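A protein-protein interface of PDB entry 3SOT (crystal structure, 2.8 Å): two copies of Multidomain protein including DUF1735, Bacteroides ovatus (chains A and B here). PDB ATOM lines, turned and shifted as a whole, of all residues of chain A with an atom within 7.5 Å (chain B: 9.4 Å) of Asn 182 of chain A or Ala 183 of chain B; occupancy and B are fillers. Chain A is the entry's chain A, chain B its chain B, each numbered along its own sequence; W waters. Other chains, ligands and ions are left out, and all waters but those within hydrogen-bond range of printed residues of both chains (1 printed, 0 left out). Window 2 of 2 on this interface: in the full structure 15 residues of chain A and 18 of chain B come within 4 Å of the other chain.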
ATOM      1  N   LYS A 170       2.805  23.838  27.350  1.00  0.00           N
ATOM      2  CA  LYS A 170       1.999  22.923  26.541  1.00  0.00           C
ATOM      3  C   LYS A 170       2.690  22.613  25.229  1.00  0.00           C
ATOM      4  O   LYS A 170       3.175  23.518  24.556  1.00  0.00           O
ATOM      5  CB  LYS A 170       0.605  23.501  26.279  1.00  0.00           C
ATOM      6  CG  LYS A 170      -0.271  23.601  27.514  1.00  0.00           C
ATOM      7  CD  LYS A 170      -1.690  23.887  27.093  1.00  0.00           C
ATOM      8  CE  LYS A 170      -2.687  23.942  28.211  1.00  0.00           C
ATOM      9  NZ  LYS A 170      -4.074  24.126  27.694  1.00  0.00           N
ATOM     10  N   VAL A 171       2.745  21.326  24.875  1.00  0.00           N
ATOM     11  CA  VAL A 171       3.380  20.840  23.647  1.00  0.00           C
ATOM     12  C   VAL A 171       2.293  20.201  22.792  1.00  0.00           C
ATOM     13  O   VAL A 171       1.760  19.151  23.146  1.00  0.00           O
ATOM     14  CB  VAL A 171       4.572  19.869  23.930  1.00  0.00           C
ATOM     15  CG1 VAL A 171       5.255  19.439  22.632  1.00  0.00           C
ATOM     16  CG2 VAL A 171       5.592  20.503  24.879  1.00  0.00           C
ATOM     17  N   TYR A 172       1.954  20.866  21.684  1.00  0.00           N
ATOM     18  CA  TYR A 172       0.919  20.440  20.737  1.00  0.00           C
ATOM     19  C   TYR A 172       1.508  19.731  19.543  1.00  0.00           C
ATOM     20  O   TYR A 172       2.448  20.237  18.946  1.00  0.00           O
ATOM     21  CB  TYR A 172       0.104  21.639  20.234  1.00  0.00           C
ATOM     22  CG  TYR A 172      -0.480  22.511  21.322  1.00  0.00           C
ATOM     23  CD1 TYR A 172      -1.744  22.263  21.831  1.00  0.00           C
ATOM     24  CD2 TYR A 172       0.203  23.634  21.783  1.00  0.00           C
ATOM     25  CE1 TYR A 172      -2.316  23.106  22.777  1.00  0.00           C
ATOM     26  CE2 TYR A 172      -0.343  24.462  22.758  1.00  0.00           C
ATOM     27  CZ  TYR A 172      -1.609  24.200  23.248  1.00  0.00           C
ATOM     28  OH  TYR A 172      -2.194  25.035  24.174  1.00  0.00           O
ATOM     29  N   THR A 173       0.942  18.579  19.169  1.00  0.00           N
ATOM     30  CA  THR A 173       1.393  17.806  18.016  1.00  0.00           C
ATOM     31  C   THR A 173       0.711  18.332  16.747  1.00  0.00           C
ATOM     32  O   THR A 173      -0.516  18.497  16.729  1.00  0.00           O
ATOM     33  CB  THR A 173       1.092  16.304  18.233  1.00  0.00           C
ATOM     34  OG1 THR A 173       1.626  15.887  19.478  1.00  0.00           O
ATOM     35  CG2 THR A 173       1.609  15.416  17.104  1.00  0.00           C
ATOM     36  N   ILE A 175      -1.031  17.848  13.563  1.00  0.00           N
ATOM     37  CA  ILE A 175      -1.856  16.849  12.910  1.00  0.00           C
ATOM     38  C   ILE A 175      -2.515  17.551  11.734  1.00  0.00           C
ATOM     39  O   ILE A 175      -3.266  18.520  11.936  1.00  0.00           O
ATOM     40  CB  ILE A 175      -2.878  16.144  13.846  1.00  0.00           C
ATOM     41  CG1 ILE A 175      -2.222  15.531  15.085  1.00  0.00           C
ATOM     42  CG2 ILE A 175      -3.648  15.093  13.068  1.00  0.00           C
ATOM     43  CD1 ILE A 175      -3.212  14.885  16.104  1.00  0.00           C
ATOM     44  N   PRO A 179      -1.478  22.589  14.536  1.00  0.00           N
ATOM     45  CA  PRO A 179      -1.324  22.014  15.887  1.00  0.00           C
ATOM     46  C   PRO A 179      -2.655  21.487  16.430  1.00  0.00           C
ATOM     47  O   PRO A 179      -3.688  22.140  16.247  1.00  0.00           O
ATOM     48  CB  PRO A 179      -0.804  23.193  16.722  1.00  0.00           C
ATOM     49  CG  PRO A 179      -0.205  24.105  15.735  1.00  0.00           C
ATOM     50  CD  PRO A 179      -1.096  24.012  14.533  1.00  0.00           C
ATOM     51  N   ASP A 180      -2.636  20.279  17.038  1.00  0.00           N
ATOM     52  CA  ASP A 180      -3.820  19.641  17.619  1.00  0.00           C
ATOM     53  C   ASP A 180      -4.292  20.427  18.861  1.00  0.00           C
ATOM     54  O   ASP A 180      -3.535  21.231  19.424  1.00  0.00           O
ATOM     55  CB  ASP A 180      -3.518  18.176  17.980  1.00  0.00           C
ATOM     56  CG  ASP A 180      -4.735  17.314  18.297  1.00  0.00           C
ATOM     57  OD1 ASP A 180      -5.697  17.344  17.521  1.00  0.00           O
ATOM     58  OD2 ASP A 180      -4.658  16.494  19.234  1.00  0.00           O
ATOM     59  N   THR A 181      -5.557  20.206  19.255  1.00  0.00           N
ATOM     60  CA  THR A 181      -6.229  20.816  20.410  1.00  0.00           C
ATOM     61  C   THR A 181      -5.662  20.223  21.711  1.00  0.00           C
ATOM     62  O   THR A 181      -5.456  20.949  22.686  1.00  0.00           O
ATOM     63  CB  THR A 181      -7.746  20.581  20.289  1.00  0.00           C
ATOM     64  OG1 THR A 181      -8.023  19.172  20.331  1.00  0.00           O
ATOM     65  CG2 THR A 181      -8.324  21.166  18.998  1.00  0.00           C
ATOM     66  N   ASN A 182      -5.400  18.902  21.705  1.00  0.00           N
ATOM     67  CA  ASN A 182      -4.817  18.167  22.823  1.00  0.00           C
ATOM     68  C   ASN A 182      -3.361  18.533  22.982  1.00  0.00           C
ATOM     69  O   ASN A 182      -2.591  18.518  22.006  1.00  0.00           O
ATOM     70  CB  ASN A 182      -4.952  16.636  22.645  1.00  0.00           C
ATOM     71  CG  ASN A 182      -6.358  16.105  22.585  1.00  0.00           C
ATOM     72  OD1 ASN A 182      -7.101  16.118  23.575  1.00  0.00           O
ATOM     73  ND2 ASN A 182      -6.709  15.534  21.446  1.00  0.00           N
ATOM     74  N   ALA A 183      -2.989  18.871  24.217  1.00  0.00           N
ATOM     75  CA  ALA A 183      -1.627  19.212  24.580  1.00  0.00           C
ATOM     76  C   ALA A 183      -1.063  18.228  25.589  1.00  0.00           C
ATOM     77  O   ALA A 183      -1.801  17.666  26.411  1.00  0.00           O
ATOM     78  CB  ALA A 183      -1.588  20.607  25.151  1.00  0.00           C
ATOM     79  N   ARG A 184       0.248  18.016  25.504  1.00  0.00           N
ATOM     80  CA  ARG A 184       1.036  17.189  26.407  1.00  0.00           C
ATOM     81  C   ARG A 184       1.893  18.087  27.275  1.00  0.00           C
ATOM     82  O   ARG A 184       2.388  19.111  26.791  1.00  0.00           O
ATOM     83  CB  ARG A 184       1.895  16.196  25.616  1.00  0.00           C
ATOM     84  CG  ARG A 184       1.241  14.865  25.377  1.00  0.00           C
ATOM     85  CD  ARG A 184       1.841  14.038  24.249  1.00  0.00           C
ATOM     86  NE  ARG A 184       3.294  13.854  24.308  1.00  0.00           N
ATOM     87  CZ  ARG A 184       4.168  14.486  23.525  1.00  0.00           C
ATOM     88  NH1 ARG A 184       3.748  15.357  22.614  1.00  0.00           N
ATOM     89  NH2 ARG A 184       5.465  14.245  23.640  1.00  0.00           N
ATOM     90  N   SER B 167       1.495   9.633  15.369  1.00  0.00           N
ATOM     91  CA  SER B 167       1.151  10.929  16.000  1.00  0.00           C
ATOM     92  C   SER B 167      -0.294  11.399  15.646  1.00  0.00           C
ATOM     93  O   SER B 167      -0.872  12.192  16.403  1.00  0.00           O
ATOM     94  CB  SER B 167       2.151  12.007  15.589  1.00  0.00           C
ATOM     95  OG  SER B 167       2.205  12.187  14.186  1.00  0.00           O
ATOM     96  N   SER B 168      -0.868  10.899  14.510  1.00  0.00           N
ATOM     97  CA  SER B 168      -2.222  11.238  14.062  1.00  0.00           C
ATOM     98  C   SER B 168      -3.231  10.137  14.460  1.00  0.00           C
ATOM     99  O   SER B 168      -4.409  10.226  14.086  1.00  0.00           O
ATOM    100  CB  SER B 168      -2.250  11.469  12.556  1.00  0.00           C
ATOM    101  OG  SER B 168      -1.463  12.595  12.207  1.00  0.00           O
ATOM    102  N   MET B 169      -2.765   9.106  15.223  1.00  0.00           N
ATOM    103  CA  MET B 169      -3.598   8.041  15.796  1.00  0.00           C
ATOM    104  C   MET B 169      -4.043   8.424  17.221  1.00  0.00           C
ATOM    105  O   MET B 169      -3.208   8.509  18.134  1.00  0.00           O
ATOM    106  CB  MET B 169      -2.897   6.689  15.817  1.00  0.00           C
ATOM    107  CG  MET B 169      -3.804   5.611  16.376  1.00  0.00           C
ATOM    108  SD  MET B 169      -3.038   3.882  16.717  1.00  0.00           S
ATOM    109  CE  MET B 169      -1.802   4.362  18.119  1.00  0.00           C
ATOM    110  N   LYS B 170      -5.342   8.680  17.393  1.00  0.00           N
ATOM    111  CA  LYS B 170      -5.932   9.081  18.670  1.00  0.00           C
ATOM    112  C   LYS B 170      -6.671   7.896  19.314  1.00  0.00           C
ATOM    113  O   LYS B 170      -7.474   7.216  18.667  1.00  0.00           O
ATOM    114  CB  LYS B 170      -6.888  10.280  18.513  1.00  0.00           C
ATOM    115  CG  LYS B 170      -6.210  11.592  18.140  1.00  0.00           C
ATOM    116  CD  LYS B 170      -7.208  12.721  18.222  1.00  0.00           C
ATOM    117  CE  LYS B 170      -6.630  14.094  18.038  1.00  0.00           C
ATOM    118  NZ  LYS B 170      -7.656  15.135  18.341  1.00  0.00           N
ATOM    119  N   VAL B 171      -6.382   7.652  20.602  1.00  0.00           N
ATOM    120  CA  VAL B 171      -6.992   6.580  21.366  1.00  0.00           C
ATOM    121  C   VAL B 171      -7.850   7.233  22.476  1.00  0.00           C
ATOM    122  O   VAL B 171      -7.322   7.831  23.425  1.00  0.00           O
ATOM    123  CB  VAL B 171      -5.948   5.571  21.915  1.00  0.00           C
ATOM    124  CG1 VAL B 171      -6.637   4.413  22.637  1.00  0.00           C
ATOM    125  CG2 VAL B 171      -5.055   5.036  20.795  1.00  0.00           C
ATOM    126  N   TYR B 172      -9.177   7.116  22.330  1.00  0.00           N
ATOM    127  CA  TYR B 172     -10.151   7.646  23.263  1.00  0.00           C
ATOM    128  C   TYR B 172     -10.636   6.585  24.222  1.00  0.00           C
ATOM    129  O   TYR B 172     -11.002   5.494  23.785  1.00  0.00           O
ATOM    130  CB  TYR B 172     -11.348   8.207  22.498  1.00  0.00           C
ATOM    131  CG  TYR B 172     -11.016   9.206  21.414  1.00  0.00           C
ATOM    132  CD1 TYR B 172     -10.942  10.567  21.694  1.00  0.00           C
ATOM    133  CD2 TYR B 172     -10.845   8.797  20.091  1.00  0.00           C
ATOM    134  CE1 TYR B 172     -10.700  11.501  20.691  1.00  0.00           C
ATOM    135  CE2 TYR B 172     -10.583   9.721  19.081  1.00  0.00           C
ATOM    136  CZ  TYR B 172     -10.518  11.080  19.386  1.00  0.00           C
ATOM    137  OH  TYR B 172     -10.292  12.029  18.416  1.00  0.00           O
ATOM    138  N   THR B 173     -10.687   6.905  25.518  1.00  0.00           N
ATOM    139  CA  THR B 173     -11.169   5.992  26.555  1.00  0.00           C
ATOM    140  C   THR B 173     -12.674   6.126  26.661  1.00  0.00           C
ATOM    141  O   THR B 173     -13.174   7.251  26.748  1.00  0.00           O
ATOM    142  CB  THR B 173     -10.472   6.286  27.907  1.00  0.00           C
ATOM    143  OG1 THR B 173      -9.068   6.230  27.726  1.00  0.00           O
ATOM    144  CG2 THR B 173     -10.876   5.334  29.010  1.00  0.00           C
ATOM    145  N   ILE B 175     -15.784   6.450  28.572  1.00  0.00           N
ATOM    146  CA  ILE B 175     -16.210   6.904  29.890  1.00  0.00           C
ATOM    147  C   ILE B 175     -17.735   7.063  29.817  1.00  0.00           C
ATOM    148  O   ILE B 175     -18.243   7.873  29.026  1.00  0.00           O
ATOM    149  CB  ILE B 175     -15.497   8.176  30.435  1.00  0.00           C
ATOM    150  CG1 ILE B 175     -13.961   8.070  30.350  1.00  0.00           C
ATOM    151  CG2 ILE B 175     -15.955   8.439  31.882  1.00  0.00           C
ATOM    152  CD1 ILE B 175     -13.183   9.331  30.793  1.00  0.00           C
ATOM    153  N   PRO B 179     -17.083   7.396  24.006  1.00  0.00           N
ATOM    154  CA  PRO B 179     -15.654   7.766  24.010  1.00  0.00           C
ATOM    155  C   PRO B 179     -15.459   9.179  24.542  1.00  0.00           C
ATOM    156  O   PRO B 179     -16.250  10.077  24.206  1.00  0.00           O
ATOM    157  CB  PRO B 179     -15.247   7.656  22.537  1.00  0.00           C
ATOM    158  CG  PRO B 179     -16.282   6.783  21.920  1.00  0.00           C
ATOM    159  CD  PRO B 179     -17.549   7.119  22.633  1.00  0.00           C
ATOM    160  N   ASP B 180     -14.439   9.364  25.406  1.00  0.00           N
ATOM    161  CA  ASP B 180     -14.114  10.657  26.009  1.00  0.00           C
ATOM    162  C   ASP B 180     -13.576  11.611  24.939  1.00  0.00           C
ATOM    163  O   ASP B 180     -13.160  11.164  23.864  1.00  0.00           O
ATOM    164  CB  ASP B 180     -13.099  10.486  27.149  1.00  0.00           C
ATOM    165  CG  ASP B 180     -12.962  11.694  28.055  1.00  0.00           C
ATOM    166  OD1 ASP B 180     -13.999  12.231  28.477  1.00  0.00           O
ATOM    167  OD2 ASP B 180     -11.815  12.008  28.461  1.00  0.00           O
ATOM    168  N   THR B 181     -13.631  12.922  25.218  1.00  0.00           N
ATOM    169  CA  THR B 181     -13.157  14.004  24.341  1.00  0.00           C
ATOM    170  C   THR B 181     -11.625  14.011  24.312  1.00  0.00           C
ATOM    171  O   THR B 181     -11.020  14.238  23.252  1.00  0.00           O
ATOM    172  CB  THR B 181     -13.717  15.337  24.823  1.00  0.00           C
ATOM    173  OG1 THR B 181     -13.236  15.591  26.153  1.00  0.00           O
ATOM    174  CG2 THR B 181     -15.242  15.361  24.784  1.00  0.00           C
ATOM    175  N   ASN B 182     -11.004  13.754  25.488  1.00  0.00           N
ATOM    176  CA  ASN B 182      -9.556  13.681  25.657  1.00  0.00           C
ATOM    177  C   ASN B 182      -9.038  12.414  25.009  1.00  0.00           C
ATOM    178  O   ASN B 182      -9.568  11.315  25.242  1.00  0.00           O
ATOM    179  CB  ASN B 182      -9.153  13.744  27.152  1.00  0.00           C
ATOM    180  CG  ASN B 182      -9.562  15.003  27.913  1.00  0.00           C
ATOM    181  OD1 ASN B 182     -10.177  14.924  28.979  1.00  0.00           O
ATOM    182  ND2 ASN B 182      -9.254  16.198  27.402  1.00  0.00           N
ATOM    183  N   ALA B 183      -8.014  12.585  24.177  1.00  0.00           N
ATOM    184  CA  ALA B 183      -7.349  11.508  23.455  1.00  0.00           C
ATOM    185  C   ALA B 183      -5.911  11.390  23.880  1.00  0.00           C
ATOM    186  O   ALA B 183      -5.289  12.374  24.257  1.00  0.00           O
ATOM    187  CB  ALA B 183      -7.429  11.745  21.966  1.00  0.00           C
ATOM    188  N   ARG B 184      -5.405  10.163  23.871  1.00  0.00           N
ATOM    189  CA  ARG B 184      -4.029   9.759  24.133  1.00  0.00           C
ATOM    190  C   ARG B 184      -3.380   9.356  22.827  1.00  0.00           C
ATOM    191  O   ARG B 184      -4.030   8.730  21.977  1.00  0.00           O
ATOM    192  CB  ARG B 184      -3.995   8.608  25.142  1.00  0.00           C
ATOM    193  CG  ARG B 184      -3.901   9.041  26.578  1.00  0.00           C
ATOM    194  CD  ARG B 184      -4.291   7.984  27.611  1.00  0.00           C
ATOM    195  NE  ARG B 184      -3.633   6.683  27.456  1.00  0.00           N
ATOM    196  CZ  ARG B 184      -4.234   5.600  26.970  1.00  0.00           C
ATOM    197  NH1 ARG B 184      -5.506   5.651  26.592  1.00  0.00           N
ATOM    198  NH2 ARG B 184      -3.574   4.452  26.875  1.00  0.00           N
ATOM    199  N   THR B 185      -2.122   9.743  22.633  1.00  0.00           N
ATOM    200  CA  THR B 185      -1.346   9.420  21.436  1.00  0.00           C
ATOM    201  C   THR B 185       0.040   8.957  21.819  1.00  0.00           C
ATOM    202  O   THR B 185       0.459   9.173  22.942  1.00  0.00           O
ATOM    203  CB  THR B 185      -1.248  10.653  20.484  1.00  0.00           C
ATOM    204  OG1 THR B 185      -0.561  11.726  21.135  1.00  0.00           O
ATOM    205  CG2 THR B 185      -2.592  11.114  19.931  1.00  0.00           C
ATOM    206  N   THR B 186       0.751   8.323  20.882  1.00  0.00           N
ATOM    207  CA  THR B 186       2.155   7.923  21.012  1.00  0.00           C
ATOM    208  C   THR B 186       2.825   8.378  19.719  1.00  0.00           C
ATOM    209  O   THR B 186       2.111   8.759  18.784  1.00  0.00           O
ATOM    210  CB  THR B 186       2.356   6.435  21.339  1.00  0.00           C
ATOM    211  OG1 THR B 186       3.730   6.272  21.661  1.00  0.00           O
ATOM    212  CG2 THR B 186       1.945   5.486  20.194  1.00  0.00           C
ATOM    213  N   LEU B 205      -2.708   1.457  22.272  1.00  0.00           N
ATOM    214  CA  LEU B 205      -1.431   1.819  22.883  1.00  0.00           C
ATOM    215  C   LEU B 205      -0.903   0.700  23.774  1.00  0.00           C
ATOM    216  O   LEU B 205      -0.016   0.958  24.600  1.00  0.00           O
ATOM    217  CB  LEU B 205      -1.584   3.121  23.702  1.00  0.00           C
ATOM    218  CG  LEU B 205      -2.073   4.369  22.932  1.00  0.00           C
ATOM    219  CD1 LEU B 205      -2.303   5.513  23.861  1.00  0.00           C
ATOM    220  CD2 LEU B 205      -1.100   4.775  21.818  1.00  0.00           C
ATOM    221  N   TYR B 294     -11.697   1.090  24.391  1.00  0.00           N
ATOM    222  CA  TYR B 294     -11.068   2.213  23.695  1.00  0.00           C
ATOM    223  C   TYR B 294     -11.567   2.363  22.280  1.00  0.00           C
ATOM    224  O   TYR B 294     -11.809   1.362  21.607  1.00  0.00           O
ATOM    225  CB  TYR B 294      -9.538   2.064  23.640  1.00  0.00           C
ATOM    226  CG  TYR B 294      -8.849   2.045  24.974  1.00  0.00           C
ATOM    227  CD1 TYR B 294      -8.566   3.232  25.654  1.00  0.00           C
ATOM    228  CD2 TYR B 294      -8.374   0.855  25.516  1.00  0.00           C
ATOM    229  CE1 TYR B 294      -7.890   3.223  26.875  1.00  0.00           C
ATOM    230  CE2 TYR B 294      -7.692   0.834  26.735  1.00  0.00           C
ATOM    231  CZ  TYR B 294      -7.425   2.024  27.399  1.00  0.00           C
ATOM    232  OH  TYR B 294      -6.729   2.007  28.594  1.00  0.00           O
ATOM    233  N   ARG B 295     -11.642   3.620  21.819  1.00  0.00           N
ATOM    234  CA  ARG B 295     -11.901   3.984  20.432  1.00  0.00           C
ATOM    235  C   ARG B 295     -10.581   4.427  19.817  1.00  0.00           C
ATOM    236  O   ARG B 295      -9.994   5.409  20.272  1.00  0.00           O
ATOM    237  CB  ARG B 295     -13.003   5.065  20.284  1.00  0.00           C
ATOM    238  CG  ARG B 295     -13.162   5.618  18.855  1.00  0.00           C
ATOM    239  CD  ARG B 295     -13.617   4.599  17.840  1.00  0.00           C
ATOM    240  NE  ARG B 295     -14.962   4.125  18.148  1.00  0.00           N
ATOM    241  CZ  ARG B 295     -16.078   4.669  17.672  1.00  0.00           C
ATOM    242  NH1 ARG B 295     -16.017   5.688  16.819  1.00  0.00           N
ATOM    243  NH2 ARG B 295     -17.260   4.170  18.008  1.00  0.00           N
ATOM    244  N   VAL B 296     -10.081   3.667  18.839  1.00  0.00           N
ATOM    245  CA  VAL B 296      -8.842   3.999  18.119  1.00  0.00           C
ATOM    246  C   VAL B 296      -9.240   4.573  16.756  1.00  0.00           C
ATOM    247  O   VAL B 296     -10.006   3.930  16.025  1.00  0.00           O
ATOM    248  CB  VAL B 296      -7.895   2.799  17.994  1.00  0.00           C
ATOM    249  CG1 VAL B 296      -6.549   3.244  17.425  1.00  0.00           C
ATOM    250  CG2 VAL B 296      -7.707   2.097  19.341  1.00  0.00           C
ATOM    251  N   ALA B 297      -8.797   5.801  16.442  1.00  0.00           N
ATOM    252  CA  ALA B 297      -9.157   6.463  15.194  1.00  0.00           C
ATOM    253  C   ALA B 297      -8.078   7.433  14.727  1.00  0.00           C
ATOM    254  O   ALA B 297      -7.561   8.226  15.520  1.00  0.00           O
ATOM    255  CB  ALA B 297     -10.462   7.213  15.368  1.00  0.00           C
HETATM  256  O   HOH W   1      -9.569  15.466  21.079  1.00  0.00           O
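NZ of Lys 170 of chain B is in salt-bridge range of OD1 of Asp 180 of chain A (3.1 Å). The side-chain amide nitrogen (ND2) of Asn 182 of chain A lies close to the side-chain amino group (NZ) of Lys 170 of chain B, at 3.3 Å.
The backbone carbonyl oxygen (O) of Thr 173 of chain A sits at hydrogen-bond distance from the backbone NH (N) of Asp 180 of chain A (2.8 Å). The side-chain carboxylate of Asp 180 of chain A sits at hydrogen-bond distance from the side-chain amide nitrogen of Asn 182 of chain A (3.2 Å). N of Lys 170 of chain B lies within hydrogen-bond range of O of Ala 297 of chain B, at 2.9 Å.
Thr 173 of chain A touches Ser 167 of chain B. Ile 175 of chain A touches Ser 167 of chain B (CD1 to O, 3.6 Å). OG of Ser 168 of chain B touches CG2 of Ile 175 of chain A, at 3.4 Å. Asn 182 of chain A touches Ala 183 of chain B.
Asn 182 of chain A touches two residues of chain B. Printed residues of chain A within 4 Å of Ala 183 of chain B: Asn 182. Asp 180 of chain A touches just one residue of chain B: Lys 170 (3.1 Å). No residue of chain B comes within 4 Å of Thr 181 of chain A. No residue of chain B comes within 4 Å of Ala 183 of chain A. Of the printed residues of chain A, Lys 170 of chain B touches Asp 180 and Asn 182. Printed residues of chain B within 4 Å of Ile 175 of chain A: Ser 167 (3.6 Å) and Ser 168 (3.4 Å). Printed residues of chain A within 4 Å of Ser 167 of chain B: Thr 173 and Ile 175. The nearest residue of chain B that does not touch Asn 182 of chain A is Asn 182 of chain B (4.04 Å).
Of the 11 printed residues of chain A, 4 touch a printed residue of chain B. Hydrophobic or aromatic side chains of chain A within 4 Å of the printed part of chain B: Ile 175. Of the 21 printed residues of chain B, 4 touch a printed residue of chain A. Printed residues of chain B that touch a printed residue of chain A: Ser 167, Ser 168, Lys 170 and Ala 183. Hydrophobic or aromatic side chains of chain B within 4 Å of the printed part of chain A: Ala 183. Among the printed residues, 6 pairs touch across the chains.
Asp 180 of chain A touches Lys 170 of chain B, but with the chains exchanged Lys 170 of chain A does not touch Asp 180 of chain B (14.4 Å). Asn 182 of chain A touches Lys 170 of chain B, but with the chains exchanged Lys 170 of chain A does not touch Asn 182 of chain B (9.5 Å). Asn 182 of chain A touches Ala 183 of chain B, but with the chains exchanged Ala 183 of chain A does not touch Asn 182 of chain B (7.5 Å). Positions printed for both chains: 170, 171, 172, 173, 175, 179, 180, 181, 182, 183 and 184. Of the 6 pairs that touch across the chains among the printed residues, none has its exchanged pair printed and touching as well.
Water W1 lies within hydrogen-bond range of the side-chain amide nitrogen of Asn 182 of chain A (2.9 Å), the backbone carbonyl oxygen of Thr 181 of chain B (2.9 Å) and the side-chain amino group of Lys 170 of chain B (3.4 Å).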
